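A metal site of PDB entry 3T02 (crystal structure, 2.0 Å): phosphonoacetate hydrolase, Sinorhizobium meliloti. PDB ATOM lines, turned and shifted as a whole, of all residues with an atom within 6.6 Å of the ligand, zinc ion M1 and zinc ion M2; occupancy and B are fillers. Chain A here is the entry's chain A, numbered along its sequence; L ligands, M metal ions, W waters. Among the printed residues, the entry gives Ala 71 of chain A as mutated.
Water W2 bridges an oxygen (O4) of the ligand and the backbone carbonyl oxygen (O) of Ile 290. Water W3 lies within hydrogen-bond range of an oxygen (O3) of the ligand (2.9 Å), the side-chain amino group of Lys 135 (3.0 Å) and the side-chain amide oxygen of Asn 72 (3.1 Å). Water W1 lies within hydrogen-bond range of OD2 of Asp 32 (2.9 Å), OD1 of Asp 214 (3.2 Å) and O3 of the ligand (3.4 Å).
Zinc ion M2 is bound by OD2 of Asp 214 (2.0 Å), NE2 of His 380 (2.0 Å), NE2 of His 218 (2.1 Å) and O5 of the ligand (2.5 Å).
Ala 71 touches zinc ion M1 (CB to ZN, 3.7 Å). Of the 25 residues printed, 5 come within 4 Å of zinc ion M1.
Residues that only touch the ligand: Phe 70 (3.5 Å). Hydrophobic or aromatic side chains within 4 Å of the ligand: Phe 70, Ala 71, His 218 and His 380. Of the 25 residues printed, 8 come within 4 Å of the ligand. The nearest printed residue that does not touch the ligand is Ile 290 (4.3 Å).
Four residues have an atom within 4 Å of zinc ion M2: Asp 214, His 218, His 254 and His 380. The nearest printed residue that does not touch zinc ion M2 is Met 256 (4.3 Å).
A ring nitrogen (ND1) of His 254 lies close to a ring nitrogen (ND1) of His 380. N of Gly 33 lies close to O of His 254 (3.4 Å). A ring nitrogen (ND1) of His 218 sits at hydrogen-bond distance from the backbone carbonyl oxygen (O) of Arg 378 (2.6 Å). The side-chain hydroxyl of Thr 212 lies within hydrogen-bond range of the backbone NH of Asp 32 (3.0 Å). ND1 of His 380 is in hydrogen-bond range of O of Ser 69 (2.8 Å). OD1 of Asp 253 is in hydrogen-bond range of N of Gly 33 (3.0 Å). The backbone carbonyl oxygen (O) of Ala 71 lies close to the side-chain amide oxygen (OD1) of Asn 75, 2.9 Å away.
The backbone NH (N) of Ala 71 sits at hydrogen-bond distance from an oxygen (O1) of the ligand (2.7 Å).
Zinc ion M1 is bound by NE2 of His 254 (1.9 Å). OD1 of Asp 32 binds zinc ion M1, 1.9 Å away. Zinc ion M1 is bound by O2 of the ligand (2.0 Å). Zinc ion M1 is bound by the side-chain carboxylate (OD2) of Asp 253, 2.2 Å away.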
ATOM      1  N   ASP A  32      15.855 -30.385 -16.150  1.00  0.00           N
ATOM      2  CA  ASP A  32      15.288 -30.011 -17.436  1.00  0.00           C
ATOM      3  C   ASP A  32      15.878 -30.844 -18.567  1.00  0.00           C
ATOM      4  O   ASP A  32      17.106 -30.925 -18.710  1.00  0.00           O
ATOM      5  CB  ASP A  32      15.560 -28.522 -17.672  1.00  0.00           C
ATOM      6  CG  ASP A  32      14.636 -27.920 -18.718  1.00  0.00           C
ATOM      7  OD1 ASP A  32      14.427 -28.533 -19.783  1.00  0.00           O
ATOM      8  OD2 ASP A  32      14.098 -26.839 -18.457  1.00  0.00           O
ATOM      9  N   GLY A  33      15.015 -31.486 -19.357  1.00  0.00           N
ATOM     10  CA  GLY A  33      15.431 -32.239 -20.547  1.00  0.00           C
ATOM     11  C   GLY A  33      16.187 -33.526 -20.265  1.00  0.00           C
ATOM     12  O   GLY A  33      16.876 -34.067 -21.146  1.00  0.00           O
ATOM     13  N   SER A  69       5.344 -31.611 -24.276  1.00  0.00           N
ATOM     14  CA  SER A  69       6.517 -31.820 -23.419  1.00  0.00           C
ATOM     15  C   SER A  69       7.517 -30.652 -23.493  1.00  0.00           C
ATOM     16  O   SER A  69       8.630 -30.811 -23.979  1.00  0.00           O
ATOM     17  CB  SER A  69       7.156 -33.210 -23.645  1.00  0.00           C
ATOM     18  OG  SER A  69       7.425 -33.499 -25.015  1.00  0.00           O
ATOM     19  N   PHE A  70       7.077 -29.486 -22.995  1.00  0.00           N
ATOM     20  CA  PHE A  70       7.923 -28.294 -22.883  1.00  0.00           C
ATOM     21  C   PHE A  70       7.961 -27.817 -21.428  1.00  0.00           C
ATOM     22  O   PHE A  70       7.149 -28.240 -20.612  1.00  0.00           O
ATOM     23  CB  PHE A  70       7.387 -27.149 -23.753  1.00  0.00           C
ATOM     24  CG  PHE A  70       7.386 -27.450 -25.235  1.00  0.00           C
ATOM     25  CD1 PHE A  70       8.574 -27.712 -25.914  1.00  0.00           C
ATOM     26  CD2 PHE A  70       6.195 -27.441 -25.955  1.00  0.00           C
ATOM     27  CE1 PHE A  70       8.573 -27.980 -27.297  1.00  0.00           C
ATOM     28  CE2 PHE A  70       6.187 -27.703 -27.338  1.00  0.00           C
ATOM     29  CZ  PHE A  70       7.385 -27.969 -28.004  1.00  0.00           C
ATOM     30  N   ALA A  71       8.901 -26.917 -21.134  1.00  0.00           N
ATOM     31  CA  ALA A  71       9.165 -26.452 -19.767  1.00  0.00           C
ATOM     32  C   ALA A  71       7.984 -25.770 -19.092  1.00  0.00           C
ATOM     33  O   ALA A  71       7.665 -26.095 -17.958  1.00  0.00           O
ATOM     34  CB  ALA A  71      10.385 -25.520 -19.755  1.00  0.00           C
ATOM     35  N   ASN A  72       7.348 -24.806 -19.759  1.00  0.00           N
ATOM     36  CA  ASN A  72       6.304 -24.033 -19.100  1.00  0.00           C
ATOM     37  C   ASN A  72       5.107 -24.865 -18.611  1.00  0.00           C
ATOM     38  O   ASN A  72       4.819 -24.830 -17.412  1.00  0.00           O
ATOM     39  CB  ASN A  72       5.873 -22.801 -19.904  1.00  0.00           C
ATOM     40  CG  ASN A  72       6.854 -21.669 -19.770  1.00  0.00           C
ATOM     41  OD1 ASN A  72       8.060 -21.883 -19.720  1.00  0.00           O
ATOM     42  ND2 ASN A  72       6.348 -20.438 -19.737  1.00  0.00           N
ATOM     43  N   PRO A  73       4.434 -25.625 -19.509  1.00  0.00           N
ATOM     44  CA  PRO A  73       3.304 -26.454 -19.022  1.00  0.00           C
ATOM     45  C   PRO A  73       3.750 -27.456 -17.931  1.00  0.00           C
ATOM     46  O   PRO A  73       3.011 -27.713 -16.973  1.00  0.00           O
ATOM     47  CB  PRO A  73       2.868 -27.242 -20.257  1.00  0.00           C
ATOM     48  CG  PRO A  73       3.483 -26.569 -21.401  1.00  0.00           C
ATOM     49  CD  PRO A  73       4.706 -25.854 -20.940  1.00  0.00           C
ATOM     50  N   ASN A  75       6.689 -27.460 -15.800  1.00  0.00           N
ATOM     51  CA  ASN A  75       7.076 -26.833 -14.522  1.00  0.00           C
ATOM     52  C   ASN A  75       5.858 -26.351 -13.751  1.00  0.00           C
ATOM     53  O   ASN A  75       5.777 -26.525 -12.526  1.00  0.00           O
ATOM     54  CB  ASN A  75       8.027 -25.657 -14.747  1.00  0.00           C
ATOM     55  CG  ASN A  75       9.461 -26.095 -14.952  1.00  0.00           C
ATOM     56  OD1 ASN A  75       9.918 -26.281 -16.095  1.00  0.00           O
ATOM     57  ND2 ASN A  75      10.174 -26.264 -13.855  1.00  0.00           N
ATOM     58  N   ASN A  92       4.366 -20.979 -24.241  1.00  0.00           N
ATOM     59  CA  ASN A  92       5.039 -19.715 -23.900  1.00  0.00           C
ATOM     60  C   ASN A  92       4.259 -18.474 -24.295  1.00  0.00           C
ATOM     61  O   ASN A  92       4.497 -17.384 -23.769  1.00  0.00           O
ATOM     62  CB  ASN A  92       6.452 -19.664 -24.501  1.00  0.00           C
ATOM     63  CG  ASN A  92       7.396 -20.634 -23.825  1.00  0.00           C
ATOM     64  OD1 ASN A  92       7.554 -20.627 -22.609  1.00  0.00           O
ATOM     65  ND2 ASN A  92       8.047 -21.471 -24.625  1.00  0.00           N
ATOM     66  N   LYS A 133      16.257 -19.971 -15.187  1.00  0.00           N
ATOM     67  CA  LYS A 133      15.792 -18.829 -15.979  1.00  0.00           C
ATOM     68  C   LYS A 133      14.784 -17.978 -15.222  1.00  0.00           C
ATOM     69  O   LYS A 133      13.958 -18.507 -14.453  1.00  0.00           O
ATOM     70  CB  LYS A 133      15.229 -19.299 -17.311  1.00  0.00           C
ATOM     71  CG  LYS A 133      16.319 -19.516 -18.370  1.00  0.00           C
ATOM     72  CD  LYS A 133      16.515 -18.296 -19.269  1.00  0.00           C
ATOM     73  CE  LYS A 133      15.760 -18.433 -20.583  1.00  0.00           C
ATOM     74  NZ  LYS A 133      16.503 -19.290 -21.563  1.00  0.00           N
ATOM     75  N   LYS A 135      12.210 -16.135 -16.334  1.00  0.00           N
ATOM     76  CA  LYS A 135      10.834 -16.096 -16.840  1.00  0.00           C
ATOM     77  C   LYS A 135       9.907 -16.979 -16.004  1.00  0.00           C
ATOM     78  O   LYS A 135       8.831 -16.559 -15.594  1.00  0.00           O
ATOM     79  CB  LYS A 135      10.762 -16.483 -18.329  1.00  0.00           C
ATOM     80  CG  LYS A 135      11.791 -17.523 -18.792  1.00  0.00           C
ATOM     81  CD  LYS A 135      11.280 -18.959 -18.764  1.00  0.00           C
ATOM     82  CE  LYS A 135      10.154 -19.176 -19.790  1.00  0.00           C
ATOM     83  NZ  LYS A 135      10.615 -19.049 -21.214  1.00  0.00           N
ATOM     84  N   THR A 212      16.011 -26.413 -13.509  1.00  0.00           N
ATOM     85  CA  THR A 212      17.212 -26.062 -14.266  1.00  0.00           C
ATOM     86  C   THR A 212      16.847 -25.720 -15.704  1.00  0.00           C
ATOM     87  O   THR A 212      15.674 -25.542 -16.006  1.00  0.00           O
ATOM     88  CB  THR A 212      18.208 -27.240 -14.238  1.00  0.00           C
ATOM     89  OG1 THR A 212      17.579 -28.417 -14.719  1.00  0.00           O
ATOM     90  CG2 THR A 212      18.697 -27.491 -12.820  1.00  0.00           C
ATOM     91  N   THR A 213      17.841 -25.587 -16.601  1.00  0.00           N
ATOM     92  CA  THR A 213      17.507 -25.492 -18.041  1.00  0.00           C
ATOM     93  C   THR A 213      18.164 -26.628 -18.806  1.00  0.00           C
ATOM     94  O   THR A 213      19.079 -27.294 -18.284  1.00  0.00           O
ATOM     95  CB  THR A 213      17.909 -24.147 -18.719  1.00  0.00           C
ATOM     96  OG1 THR A 213      19.324 -24.129 -18.964  1.00  0.00           O
ATOM     97  CG2 THR A 213      17.488 -22.938 -17.902  1.00  0.00           C
ATOM     98  N   ASP A 214      17.706 -26.858 -20.030  1.00  0.00           N
ATOM     99  CA  ASP A 214      18.226 -27.964 -20.833  1.00  0.00           C
ATOM    100  C   ASP A 214      19.242 -27.540 -21.924  1.00  0.00           C
ATOM    101  O   ASP A 214      19.345 -28.186 -22.969  1.00  0.00           O
ATOM    102  CB  ASP A 214      17.083 -28.786 -21.429  1.00  0.00           C
ATOM    103  CG  ASP A 214      16.161 -27.949 -22.319  1.00  0.00           C
ATOM    104  OD1 ASP A 214      16.337 -26.722 -22.428  1.00  0.00           O
ATOM    105  OD2 ASP A 214      15.245 -28.541 -22.913  1.00  0.00           O
ATOM    106  N   TYR A 215      19.973 -26.464 -21.650  1.00  0.00           N
ATOM    107  CA  TYR A 215      21.060 -26.014 -22.520  1.00  0.00           C
ATOM    108  C   TYR A 215      22.025 -27.141 -22.918  1.00  0.00           C
ATOM    109  O   TYR A 215      22.284 -27.355 -24.113  1.00  0.00           O
ATOM    110  CB  TYR A 215      21.830 -24.864 -21.870  1.00  0.00           C
ATOM    111  CG  TYR A 215      23.129 -24.554 -22.607  1.00  0.00           C
ATOM    112  CD1 TYR A 215      23.124 -23.795 -23.779  1.00  0.00           C
ATOM    113  CD2 TYR A 215      24.348 -25.048 -22.137  1.00  0.00           C
ATOM    114  CE1 TYR A 215      24.291 -23.526 -24.473  1.00  0.00           C
ATOM    115  CE2 TYR A 215      25.529 -24.779 -22.826  1.00  0.00           C
ATOM    116  CZ  TYR A 215      25.490 -24.016 -23.984  1.00  0.00           C
ATOM    117  OH  TYR A 215      26.665 -23.755 -24.656  1.00  0.00           O
ATOM    118  N   HIS A 218      20.172 -30.066 -25.088  1.00  0.00           N
ATOM    119  CA  HIS A 218      19.885 -29.699 -26.490  1.00  0.00           C
ATOM    120  C   HIS A 218      21.165 -29.806 -27.352  1.00  0.00           C
ATOM    121  O   HIS A 218      21.088 -30.050 -28.560  1.00  0.00           O
ATOM    122  CB  HIS A 218      19.334 -28.268 -26.577  1.00  0.00           C
ATOM    123  CG  HIS A 218      17.846 -28.169 -26.457  1.00  0.00           C
ATOM    124  ND1 HIS A 218      16.994 -28.629 -27.431  1.00  0.00           N
ATOM    125  CD2 HIS A 218      17.056 -27.602 -25.512  1.00  0.00           C
ATOM    126  CE1 HIS A 218      15.745 -28.381 -27.080  1.00  0.00           C
ATOM    127  NE2 HIS A 218      15.754 -27.756 -25.919  1.00  0.00           N
ATOM    128  N   ASP A 253      11.034 -32.070 -16.612  1.00  0.00           N
ATOM    129  CA  ASP A 253       9.898 -31.519 -17.329  1.00  0.00           C
ATOM    130  C   ASP A 253       9.569 -32.260 -18.648  1.00  0.00           C
ATOM    131  O   ASP A 253       8.424 -32.231 -19.111  1.00  0.00           O
ATOM    132  CB  ASP A 253      10.096 -30.009 -17.566  1.00  0.00           C
ATOM    133  CG  ASP A 253      11.333 -29.680 -18.416  1.00  0.00           C
ATOM    134  OD1 ASP A 253      12.246 -30.519 -18.602  1.00  0.00           O
ATOM    135  OD2 ASP A 253      11.384 -28.539 -18.888  1.00  0.00           O
ATOM    136  N   HIS A 254      10.569 -32.924 -19.217  1.00  0.00           N
ATOM    137  CA  HIS A 254      10.464 -33.651 -20.495  1.00  0.00           C
ATOM    138  C   HIS A 254      11.809 -34.300 -20.766  1.00  0.00           C
ATOM    139  O   HIS A 254      12.800 -33.973 -20.120  1.00  0.00           O
ATOM    140  CB  HIS A 254      10.103 -32.697 -21.642  1.00  0.00           C
ATOM    141  CG  HIS A 254      11.055 -31.548 -21.775  1.00  0.00           C
ATOM    142  ND1 HIS A 254      12.312 -31.680 -22.321  1.00  0.00           N
ATOM    143  CD2 HIS A 254      10.940 -30.251 -21.402  1.00  0.00           C
ATOM    144  CE1 HIS A 254      12.930 -30.519 -22.282  1.00  0.00           C
ATOM    145  NE2 HIS A 254      12.132 -29.638 -21.726  1.00  0.00           N
ATOM    146  N   GLY A 255      11.838 -35.243 -21.706  1.00  0.00           N
ATOM    147  CA  GLY A 255      13.081 -35.853 -22.127  1.00  0.00           C
ATOM    148  C   GLY A 255      13.633 -35.122 -23.330  1.00  0.00           C
ATOM    149  O   GLY A 255      13.371 -33.926 -23.532  1.00  0.00           O
ATOM    150  N   MET A 256      14.399 -35.849 -24.144  1.00  0.00           N
ATOM    151  CA  MET A 256      15.178 -35.224 -25.216  1.00  0.00           C
ATOM    152  C   MET A 256      15.554 -36.287 -26.227  1.00  0.00           C
ATOM    153  O   MET A 256      15.999 -37.364 -25.851  1.00  0.00           O
ATOM    154  CB  MET A 256      16.451 -34.591 -24.630  1.00  0.00           C
ATOM    155  CG  MET A 256      17.233 -33.693 -25.597  1.00  0.00           C
ATOM    156  SD  MET A 256      16.342 -32.196 -26.069  1.00  0.00           S
ATOM    157  CE  MET A 256      16.643 -31.156 -24.641  1.00  0.00           C
ATOM    158  N   ILE A 290       6.900 -23.731 -28.113  1.00  0.00           N
ATOM    159  CA  ILE A 290       8.273 -23.793 -27.574  1.00  0.00           C
ATOM    160  C   ILE A 290       8.934 -22.420 -27.437  1.00  0.00           C
ATOM    161  O   ILE A 290       9.773 -22.214 -26.562  1.00  0.00           O
ATOM    162  CB  ILE A 290       9.194 -24.740 -28.406  1.00  0.00           C
ATOM    163  CG1 ILE A 290      10.552 -24.937 -27.719  1.00  0.00           C
ATOM    164  CG2 ILE A 290       9.358 -24.242 -29.859  1.00  0.00           C
ATOM    165  CD1 ILE A 290      11.413 -26.075 -28.260  1.00  0.00           C
ATOM    166  N   GLY A 299      16.288 -22.708 -31.554  1.00  0.00           N
ATOM    167  CA  GLY A 299      15.670 -23.025 -30.263  1.00  0.00           C
ATOM    168  C   GLY A 299      14.153 -22.838 -30.340  1.00  0.00           C
ATOM    169  O   GLY A 299      13.469 -22.801 -29.320  1.00  0.00           O
ATOM    170  N   ARG A 378      18.585 -31.420 -31.436  1.00  0.00           N
ATOM    171  CA  ARG A 378      17.993 -32.270 -30.411  1.00  0.00           C
ATOM    172  C   ARG A 378      16.836 -31.470 -29.796  1.00  0.00           C
ATOM    173  O   ARG A 378      16.993 -30.294 -29.483  1.00  0.00           O
ATOM    174  CB  ARG A 378      19.010 -32.620 -29.336  1.00  0.00           C
ATOM    175  CG  ARG A 378      20.247 -33.370 -29.831  1.00  0.00           C
ATOM    176  CD  ARG A 378      21.268 -33.611 -28.699  1.00  0.00           C
ATOM    177  NE  ARG A 378      20.682 -34.282 -27.533  1.00  0.00           N
ATOM    178  CZ  ARG A 378      20.267 -35.553 -27.508  1.00  0.00           C
ATOM    179  NH1 ARG A 378      20.343 -36.306 -28.604  1.00  0.00           N
ATOM    180  NH2 ARG A 378      19.749 -36.054 -26.397  1.00  0.00           N
ATOM    181  N   SER A 379      15.682 -32.112 -29.616  1.00  0.00           N
ATOM    182  CA  SER A 379      14.530 -31.409 -29.061  1.00  0.00           C
ATOM    183  C   SER A 379      13.471 -32.299 -28.420  1.00  0.00           C
ATOM    184  O   SER A 379      13.703 -33.492 -28.168  1.00  0.00           O
ATOM    185  CB  SER A 379      13.899 -30.495 -30.125  1.00  0.00           C
ATOM    186  OG  SER A 379      13.340 -29.346 -29.509  1.00  0.00           O
ATOM    187  N   HIS A 380      12.293 -31.708 -28.209  1.00  0.00           N
ATOM    188  CA  HIS A 380      11.212 -32.312 -27.429  1.00  0.00           C
ATOM    189  C   HIS A 380       9.867 -31.655 -27.783  1.00  0.00           C
ATOM    190  O   HIS A 380       9.781 -30.837 -28.718  1.00  0.00           O
ATOM    191  CB  HIS A 380      11.510 -32.190 -25.924  1.00  0.00           C
ATOM    192  CG  HIS A 380      11.956 -30.813 -25.525  1.00  0.00           C
ATOM    193  ND1 HIS A 380      11.104 -29.888 -24.962  1.00  0.00           N
ATOM    194  CD2 HIS A 380      13.149 -30.197 -25.637  1.00  0.00           C
ATOM    195  CE1 HIS A 380      11.753 -28.763 -24.735  1.00  0.00           C
ATOM    196  NE2 HIS A 380      13.016 -28.926 -25.131  1.00  0.00           N
HETATM  197  P1  LIG L   1      12.163 -25.669 -22.664  1.00  0.00           P
HETATM  198  O1  LIG L   1      10.751 -26.152 -22.924  1.00  0.00           O
HETATM  199  O2  LIG L   1      12.960 -26.524 -21.706  1.00  0.00           O
HETATM  200  O3  LIG L   1      12.234 -24.193 -22.294  1.00  0.00           O
HETATM  201  C1  LIG L   1      12.956 -25.777 -24.270  1.00  0.00           C
HETATM  202  C2  LIG L   1      14.050 -24.761 -24.359  1.00  0.00           C
HETATM  203  O4  LIG L   1      13.745 -23.570 -24.564  1.00  0.00           O
HETATM  204  O5  LIG L   1      15.226 -25.166 -24.230  1.00  0.00           O
HETATM  205 ZN    ZN M   1      12.729 -28.190 -20.639  1.00  0.00          ZN
HETATM  206 ZN    ZN M   2      14.301 -27.522 -24.403  1.00  0.00          ZN
HETATM  207  O   HOH W   1      14.905 -24.833 -20.338  1.00  0.00           O
HETATM  208  O   HOH W   2      11.992 -21.703 -24.551  1.00  0.00           O
HETATM  209  O   HOH W   3      10.882 -21.991 -21.067  1.00  0.00           O
